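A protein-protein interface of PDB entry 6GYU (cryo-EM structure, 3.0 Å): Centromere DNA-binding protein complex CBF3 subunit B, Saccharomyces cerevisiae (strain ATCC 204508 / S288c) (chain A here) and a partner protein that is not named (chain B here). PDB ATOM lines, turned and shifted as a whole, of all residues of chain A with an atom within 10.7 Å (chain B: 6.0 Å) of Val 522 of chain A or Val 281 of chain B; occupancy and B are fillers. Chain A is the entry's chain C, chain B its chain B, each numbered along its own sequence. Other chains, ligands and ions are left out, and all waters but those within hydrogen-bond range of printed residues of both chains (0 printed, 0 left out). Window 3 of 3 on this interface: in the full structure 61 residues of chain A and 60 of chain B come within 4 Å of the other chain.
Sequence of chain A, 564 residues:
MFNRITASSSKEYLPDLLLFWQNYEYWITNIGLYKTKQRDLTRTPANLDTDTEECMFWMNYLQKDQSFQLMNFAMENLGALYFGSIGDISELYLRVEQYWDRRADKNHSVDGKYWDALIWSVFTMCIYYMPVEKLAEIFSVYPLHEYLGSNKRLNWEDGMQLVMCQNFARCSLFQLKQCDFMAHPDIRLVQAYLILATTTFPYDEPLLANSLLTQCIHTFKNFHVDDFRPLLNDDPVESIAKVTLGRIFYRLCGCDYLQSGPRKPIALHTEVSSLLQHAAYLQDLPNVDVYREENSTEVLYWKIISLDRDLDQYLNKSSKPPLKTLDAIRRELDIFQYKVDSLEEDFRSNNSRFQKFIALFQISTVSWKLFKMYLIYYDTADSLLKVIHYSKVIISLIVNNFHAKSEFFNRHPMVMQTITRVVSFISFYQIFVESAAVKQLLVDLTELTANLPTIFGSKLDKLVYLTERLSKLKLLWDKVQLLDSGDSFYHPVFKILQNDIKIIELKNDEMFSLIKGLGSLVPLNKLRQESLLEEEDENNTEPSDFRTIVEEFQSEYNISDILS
CE of Met 511 of chain A touches OE2 of Glu 282 of chain B, at 3.6 Å. Met 511 of chain A touches Lys 286 of chain B (CE to CG, 3.8 Å). Leu 514 of chain A touches Ala 285 of chain B (CD2 to CB, 3.7 Å). Ile 515 of chain A touches Val 281 of chain B. CG1 of Ile 515 of chain A touches CB of Ala 285 of chain B (3.9 Å). Leu 518 of chain A touches Ala 285 of chain B. CB of Leu 521 of chain A touches CG1 of Val 281 of chain B (3.9 Å). Val 522 of chain A touches Val 281 of chain B.
Of chain B, only Val 281 (3.96 Å) comes within 4 Å of Val 522 of chain A. Val 281 of chain B touches just these residues of chain A: Ile 515 (3.7 Å), Leu 521 (3.9 Å) and Val 522 (3.96 Å). No residue of chain A comes within 4 Å of Asp 279 of chain B. No residue of chain A comes within 4 Å of Ile 284 of chain B. Of the printed residues of chain A, Ala 285 of chain B touches Leu 514 (3.7 Å), Ile 515 (3.9 Å) and Leu 518 (3.8 Å). Of the printed residues of chain B, Ile 515 of chain A touches Val 281 and Ala 285. Printed residues of chain A within 4 Å of Glu 282 of chain B: Met 511 (3.6 Å). Ser 520 of chain A touches none of the printed residues of chain B. The nearest residue of chain B that does not touch Val 522 of chain A is Asp 279 of chain B (5.7 Å). The nearest residue of chain A that does not touch Val 281 of chain B is Pro 523 of chain A (5.1 Å). The nearest printed residue of chain A that does not touch Lys 286 of chain B is Leu 514 of chain A (5.1 Å).
Hydrophobic or aromatic side chains of chain B within 4 Å of the printed part of chain A: Val 281 and Ala 285. Printed residues of chain A that touch a printed residue of chain B: Met 511, Leu 514, Ile 515, Leu 518, Leu 521 and Val 522. Hydrophobic or aromatic side chains of chain A within 4 Å of the printed part of chain B: Met 511, Leu 514, Ile 515, Leu 518 and Leu 521. Among the printed residues, no Asp or Glu carboxylate lies within 4 Å of a Lys or Arg side-chain nitrogen of the other chain.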
ATOM      1  N   THR A  42      -3.564  -0.006  14.545  1.00  0.00           N
ATOM      2  CA  THR A  42      -2.519  -0.697  13.799  1.00  0.00           C
ATOM      3  C   THR A  42      -1.273   0.168  13.671  1.00  0.00           C
ATOM      4  O   THR A  42      -0.189  -0.336  13.357  1.00  0.00           O
ATOM      5  CB  THR A  42      -3.036  -1.093  12.418  1.00  0.00           C
ATOM      6  OG1 THR A  42      -3.378   0.087  11.683  1.00  0.00           O
ATOM      7  CG2 THR A  42      -4.265  -1.969  12.545  1.00  0.00           C
ATOM      8  N   MET A 511     -18.394   2.573  15.234  1.00  0.00           N
ATOM      9  CA  MET A 511     -18.776   1.368  14.510  1.00  0.00           C
ATOM     10  C   MET A 511     -17.617   0.824  13.686  1.00  0.00           C
ATOM     11  O   MET A 511     -17.426  -0.394  13.608  1.00  0.00           O
ATOM     12  CB  MET A 511     -19.983   1.649  13.618  1.00  0.00           C
ATOM     13  CG  MET A 511     -20.518   0.429  12.889  1.00  0.00           C
ATOM     14  SD  MET A 511     -21.122  -0.853  14.002  1.00  0.00           S
ATOM     15  CE  MET A 511     -22.628  -0.093  14.592  1.00  0.00           C
ATOM     16  N   PHE A 512     -16.820   1.705  13.080  1.00  0.00           N
ATOM     17  CA  PHE A 512     -15.698   1.242  12.273  1.00  0.00           C
ATOM     18  C   PHE A 512     -14.573   0.691  13.133  1.00  0.00           C
ATOM     19  O   PHE A 512     -13.916  -0.278  12.737  1.00  0.00           O
ATOM     20  CB  PHE A 512     -15.190   2.374  11.383  1.00  0.00           C
ATOM     21  CG  PHE A 512     -16.183   2.810  10.348  1.00  0.00           C
ATOM     22  CD1 PHE A 512     -16.365   2.069   9.190  1.00  0.00           C
ATOM     23  CD2 PHE A 512     -16.943   3.954  10.537  1.00  0.00           C
ATOM     24  CE1 PHE A 512     -17.286   2.464   8.235  1.00  0.00           C
ATOM     25  CE2 PHE A 512     -17.866   4.357   9.586  1.00  0.00           C
ATOM     26  CZ  PHE A 512     -18.036   3.611   8.434  1.00  0.00           C
ATOM     27  N   SER A 513     -14.364   1.263  14.320  1.00  0.00           N
ATOM     28  CA  SER A 513     -13.433   0.671  15.273  1.00  0.00           C
ATOM     29  C   SER A 513     -13.940  -0.668  15.786  1.00  0.00           C
ATOM     30  O   SER A 513     -13.141  -1.566  16.057  1.00  0.00           O
ATOM     31  CB  SER A 513     -13.190   1.625  16.438  1.00  0.00           C
ATOM     32  OG  SER A 513     -14.372   1.798  17.197  1.00  0.00           O
ATOM     33  N   LEU A 514     -15.262  -0.831  15.882  1.00  0.00           N
ATOM     34  CA  LEU A 514     -15.839  -2.119  16.254  1.00  0.00           C
ATOM     35  C   LEU A 514     -15.589  -3.163  15.173  1.00  0.00           C
ATOM     36  O   LEU A 514     -15.248  -4.313  15.479  1.00  0.00           O
ATOM     37  CB  LEU A 514     -17.334  -1.947  16.507  1.00  0.00           C
ATOM     38  CG  LEU A 514     -18.211  -2.986  17.202  1.00  0.00           C
ATOM     39  CD1 LEU A 514     -19.336  -2.238  17.837  1.00  0.00           C
ATOM     40  CD2 LEU A 514     -18.788  -3.999  16.257  1.00  0.00           C
ATOM     41  N   ILE A 515     -15.752  -2.776  13.906  1.00  0.00           N
ATOM     42  CA  ILE A 515     -15.520  -3.690  12.791  1.00  0.00           C
ATOM     43  C   ILE A 515     -14.042  -4.064  12.704  1.00  0.00           C
ATOM     44  O   ILE A 515     -13.693  -5.229  12.475  1.00  0.00           O
ATOM     45  CB  ILE A 515     -16.033  -3.066  11.480  1.00  0.00           C
ATOM     46  CG1 ILE A 515     -17.550  -2.906  11.527  1.00  0.00           C
ATOM     47  CG2 ILE A 515     -15.673  -3.908  10.286  1.00  0.00           C
ATOM     48  CD1 ILE A 515     -18.097  -2.066  10.401  1.00  0.00           C
ATOM     49  N   LYS A 516     -13.154  -3.093  12.929  1.00  0.00           N
ATOM     50  CA  LYS A 516     -11.724  -3.392  12.955  1.00  0.00           C
ATOM     51  C   LYS A 516     -11.348  -4.234  14.170  1.00  0.00           C
ATOM     52  O   LYS A 516     -10.364  -4.980  14.136  1.00  0.00           O
ATOM     53  CB  LYS A 516     -10.913  -2.097  12.932  1.00  0.00           C
ATOM     54  CG  LYS A 516     -10.991  -1.333  11.623  1.00  0.00           C
ATOM     55  CD  LYS A 516     -10.170  -0.059  11.684  1.00  0.00           C
ATOM     56  CE  LYS A 516     -10.173   0.667  10.348  1.00  0.00           C
ATOM     57  NZ  LYS A 516     -11.520   1.195   9.995  1.00  0.00           N
ATOM     58  N   GLY A 517     -12.125  -4.134  15.251  1.00  0.00           N
ATOM     59  CA  GLY A 517     -11.825  -4.919  16.435  1.00  0.00           C
ATOM     60  C   GLY A 517     -12.320  -6.348  16.347  1.00  0.00           C
ATOM     61  O   GLY A 517     -11.764  -7.244  16.984  1.00  0.00           O
ATOM     62  N   LEU A 518     -13.377  -6.587  15.564  1.00  0.00           N
ATOM     63  CA  LEU A 518     -13.913  -7.944  15.485  1.00  0.00           C
ATOM     64  C   LEU A 518     -13.053  -8.845  14.608  1.00  0.00           C
ATOM     65  O   LEU A 518     -13.115 -10.073  14.726  1.00  0.00           O
ATOM     66  CB  LEU A 518     -15.352  -7.932  14.980  1.00  0.00           C
ATOM     67  CG  LEU A 518     -16.393  -7.372  15.943  1.00  0.00           C
ATOM     68  CD1 LEU A 518     -17.756  -7.431  15.302  1.00  0.00           C
ATOM     69  CD2 LEU A 518     -16.383  -8.126  17.249  1.00  0.00           C
ATOM     70  N   GLY A 519     -12.247  -8.265  13.724  1.00  0.00           N
ATOM     71  CA  GLY A 519     -11.289  -9.075  12.997  1.00  0.00           C
ATOM     72  C   GLY A 519     -11.382  -9.054  11.489  1.00  0.00           C
ATOM     73  O   GLY A 519     -11.094  -8.036  10.854  1.00  0.00           O
ATOM     74  N   SER A 520     -11.787 -10.189  10.905  1.00  0.00           N
ATOM     75  CA  SER A 520     -11.778 -10.334   9.452  1.00  0.00           C
ATOM     76  C   SER A 520     -12.892  -9.524   8.798  1.00  0.00           C
ATOM     77  O   SER A 520     -12.902  -9.346   7.575  1.00  0.00           O
ATOM     78  CB  SER A 520     -11.893 -11.809   9.069  1.00  0.00           C
ATOM     79  OG  SER A 520     -10.764 -12.540   9.515  1.00  0.00           O
ATOM     80  N   LEU A 521     -13.855  -9.058   9.593  1.00  0.00           N
ATOM     81  CA  LEU A 521     -14.760  -8.015   9.136  1.00  0.00           C
ATOM     82  C   LEU A 521     -13.964  -6.752   8.842  1.00  0.00           C
ATOM     83  O   LEU A 521     -13.314  -6.192   9.729  1.00  0.00           O
ATOM     84  CB  LEU A 521     -15.827  -7.744  10.196  1.00  0.00           C
ATOM     85  CG  LEU A 521     -16.773  -8.907  10.502  1.00  0.00           C
ATOM     86  CD1 LEU A 521     -17.687  -8.562  11.665  1.00  0.00           C
ATOM     87  CD2 LEU A 521     -17.583  -9.283   9.270  1.00  0.00           C
ATOM     88  N   VAL A 522     -13.985  -6.325   7.585  1.00  0.00           N
ATOM     89  CA  VAL A 522     -13.181  -5.188   7.144  1.00  0.00           C
ATOM     90  C   VAL A 522     -14.095  -4.139   6.514  1.00  0.00           C
ATOM     91  O   VAL A 522     -15.007  -4.483   5.746  1.00  0.00           O
ATOM     92  CB  VAL A 522     -12.045  -5.653   6.208  1.00  0.00           C
ATOM     93  CG1 VAL A 522     -12.571  -6.437   5.003  1.00  0.00           C
ATOM     94  CG2 VAL A 522     -11.186  -4.479   5.750  1.00  0.00           C
ATOM     95  N   PRO A 523     -13.942  -2.862   6.862  1.00  0.00           N
ATOM     96  CA  PRO A 523     -14.727  -1.825   6.183  1.00  0.00           C
ATOM     97  C   PRO A 523     -14.169  -1.537   4.799  1.00  0.00           C
ATOM     98  O   PRO A 523     -12.954  -1.536   4.583  1.00  0.00           O
ATOM     99  CB  PRO A 523     -14.593  -0.613   7.110  1.00  0.00           C
ATOM    100  CG  PRO A 523     -13.304  -0.831   7.820  1.00  0.00           C
ATOM    101  CD  PRO A 523     -13.176  -2.318   7.998  1.00  0.00           C
ATOM    102  N   LEU A 524     -15.075  -1.298   3.853  1.00  0.00           N
ATOM    103  CA  LEU A 524     -14.702  -1.003   2.478  1.00  0.00           C
ATOM    104  C   LEU A 524     -14.722   0.481   2.150  1.00  0.00           C
ATOM    105  O   LEU A 524     -13.803   0.963   1.485  1.00  0.00           O
ATOM    106  CB  LEU A 524     -15.625  -1.737   1.494  1.00  0.00           C
ATOM    107  N   ASN A 525     -15.737   1.210   2.599  1.00  0.00           N
ATOM    108  CA  ASN A 525     -15.840   2.637   2.321  1.00  0.00           C
ATOM    109  C   ASN A 525     -14.995   3.449   3.297  1.00  0.00           C
ATOM    110  O   ASN A 525     -14.193   4.290   2.889  1.00  0.00           O
ATOM    111  CB  ASN A 525     -17.299   3.090   2.382  1.00  0.00           C
ATOM    112  CG  ASN A 525     -18.128   2.540   1.238  1.00  0.00           C
ATOM    113  OD1 ASN A 525     -17.679   2.506   0.093  1.00  0.00           O
ATOM    114  ND2 ASN A 525     -19.344   2.105   1.544  1.00  0.00           N
ATOM    115  N   ASP B 279     -24.671  -1.222   6.267  1.00  0.00           N
ATOM    116  CA  ASP B 279     -23.651  -2.014   5.601  1.00  0.00           C
ATOM    117  C   ASP B 279     -23.831  -3.479   5.996  1.00  0.00           C
ATOM    118  O   ASP B 279     -24.081  -3.771   7.171  1.00  0.00           O
ATOM    119  CB  ASP B 279     -22.272  -1.496   6.032  1.00  0.00           C
ATOM    120  CG  ASP B 279     -21.125  -1.988   5.160  1.00  0.00           C
ATOM    121  OD1 ASP B 279     -21.344  -2.712   4.176  1.00  0.00           O
ATOM    122  OD2 ASP B 279     -19.970  -1.635   5.476  1.00  0.00           O
ATOM    123  N   PRO B 280     -23.769  -4.421   5.046  1.00  0.00           N
ATOM    124  CA  PRO B 280     -23.807  -5.847   5.423  1.00  0.00           C
ATOM    125  C   PRO B 280     -22.660  -6.309   6.314  1.00  0.00           C
ATOM    126  O   PRO B 280     -22.790  -7.354   6.962  1.00  0.00           O
ATOM    127  CB  PRO B 280     -23.783  -6.561   4.067  1.00  0.00           C
ATOM    128  CG  PRO B 280     -24.469  -5.613   3.166  1.00  0.00           C
ATOM    129  CD  PRO B 280     -24.077  -4.236   3.618  1.00  0.00           C
ATOM    130  N   VAL B 281     -21.549  -5.576   6.374  1.00  0.00           N
ATOM    131  CA  VAL B 281     -20.540  -5.848   7.389  1.00  0.00           C
ATOM    132  C   VAL B 281     -20.998  -5.315   8.743  1.00  0.00           C
ATOM    133  O   VAL B 281     -20.802  -5.963   9.780  1.00  0.00           O
ATOM    134  CB  VAL B 281     -19.193  -5.242   6.953  1.00  0.00           C
ATOM    135  CG1 VAL B 281     -18.116  -5.516   7.979  1.00  0.00           C
ATOM    136  CG2 VAL B 281     -18.790  -5.788   5.597  1.00  0.00           C
ATOM    137  N   GLU B 282     -21.645  -4.143   8.742  1.00  0.00           N
ATOM    138  CA  GLU B 282     -22.156  -3.534   9.967  1.00  0.00           C
ATOM    139  C   GLU B 282     -23.268  -4.365  10.599  1.00  0.00           C
ATOM    140  O   GLU B 282     -23.390  -4.399  11.828  1.00  0.00           O
ATOM    141  CB  GLU B 282     -22.651  -2.118   9.663  1.00  0.00           C
ATOM    142  CG  GLU B 282     -23.156  -1.326  10.854  1.00  0.00           C
ATOM    143  CD  GLU B 282     -23.618   0.065  10.471  1.00  0.00           C
ATOM    144  OE1 GLU B 282     -23.543   0.404   9.271  1.00  0.00           O
ATOM    145  OE2 GLU B 282     -24.062   0.815  11.366  1.00  0.00           O
ATOM    146  N   SER B 283     -24.059  -5.065   9.782  1.00  0.00           N
ATOM    147  CA  SER B 283     -25.120  -5.917  10.313  1.00  0.00           C
ATOM    148  C   SER B 283     -24.553  -7.101  11.089  1.00  0.00           C
ATOM    149  O   SER B 283     -25.003  -7.392  12.205  1.00  0.00           O
ATOM    150  CB  SER B 283     -26.007  -6.402   9.170  1.00  0.00           C
ATOM    151  OG  SER B 283     -26.680  -5.316   8.560  1.00  0.00           O
ATOM    152  N   ILE B 284     -23.546  -7.773  10.526  1.00  0.00           N
ATOM    153  CA  ILE B 284     -22.895  -8.883  11.212  1.00  0.00           C
ATOM    154  C   ILE B 284     -22.125  -8.378  12.427  1.00  0.00           C
ATOM    155  O   ILE B 284     -22.058  -9.060  13.463  1.00  0.00           O
ATOM    156  CB  ILE B 284     -21.996  -9.634  10.214  1.00  0.00           C
ATOM    157  CG1 ILE B 284     -22.831 -10.121   9.031  1.00  0.00           C
ATOM    158  CG2 ILE B 284     -21.318 -10.830  10.858  1.00  0.00           C
ATOM    159  CD1 ILE B 284     -22.007 -10.627   7.871  1.00  0.00           C
ATOM    160  N   ALA B 285     -21.588  -7.156  12.344  1.00  0.00           N
ATOM    161  CA  ALA B 285     -20.918  -6.547  13.489  1.00  0.00           C
ATOM    162  C   ALA B 285     -21.890  -6.284  14.633  1.00  0.00           C
ATOM    163  O   ALA B 285     -21.560  -6.523  15.799  1.00  0.00           O
ATOM    164  CB  ALA B 285     -20.233  -5.253  13.061  1.00  0.00           C
ATOM    165  N   LYS B 286     -23.106  -5.832  14.320  1.00  0.00           N
ATOM    166  CA  LYS B 286     -24.084  -5.599  15.377  1.00  0.00           C
ATOM    167  C   LYS B 286     -24.657  -6.898  15.924  1.00  0.00           C
ATOM    168  O   LYS B 286     -25.020  -6.953  17.102  1.00  0.00           O
ATOM    169  CB  LYS B 286     -25.206  -4.690  14.886  1.00  0.00           C
ATOM    170  CG  LYS B 286     -24.771  -3.258  14.675  1.00  0.00           C
ATOM    171  CD  LYS B 286     -25.961  -2.344  14.496  1.00  0.00           C
ATOM    172  CE  LYS B 286     -26.608  -2.547  13.150  1.00  0.00           C
ATOM    173  NZ  LYS B 286     -27.700  -1.564  12.918  1.00  0.00           N
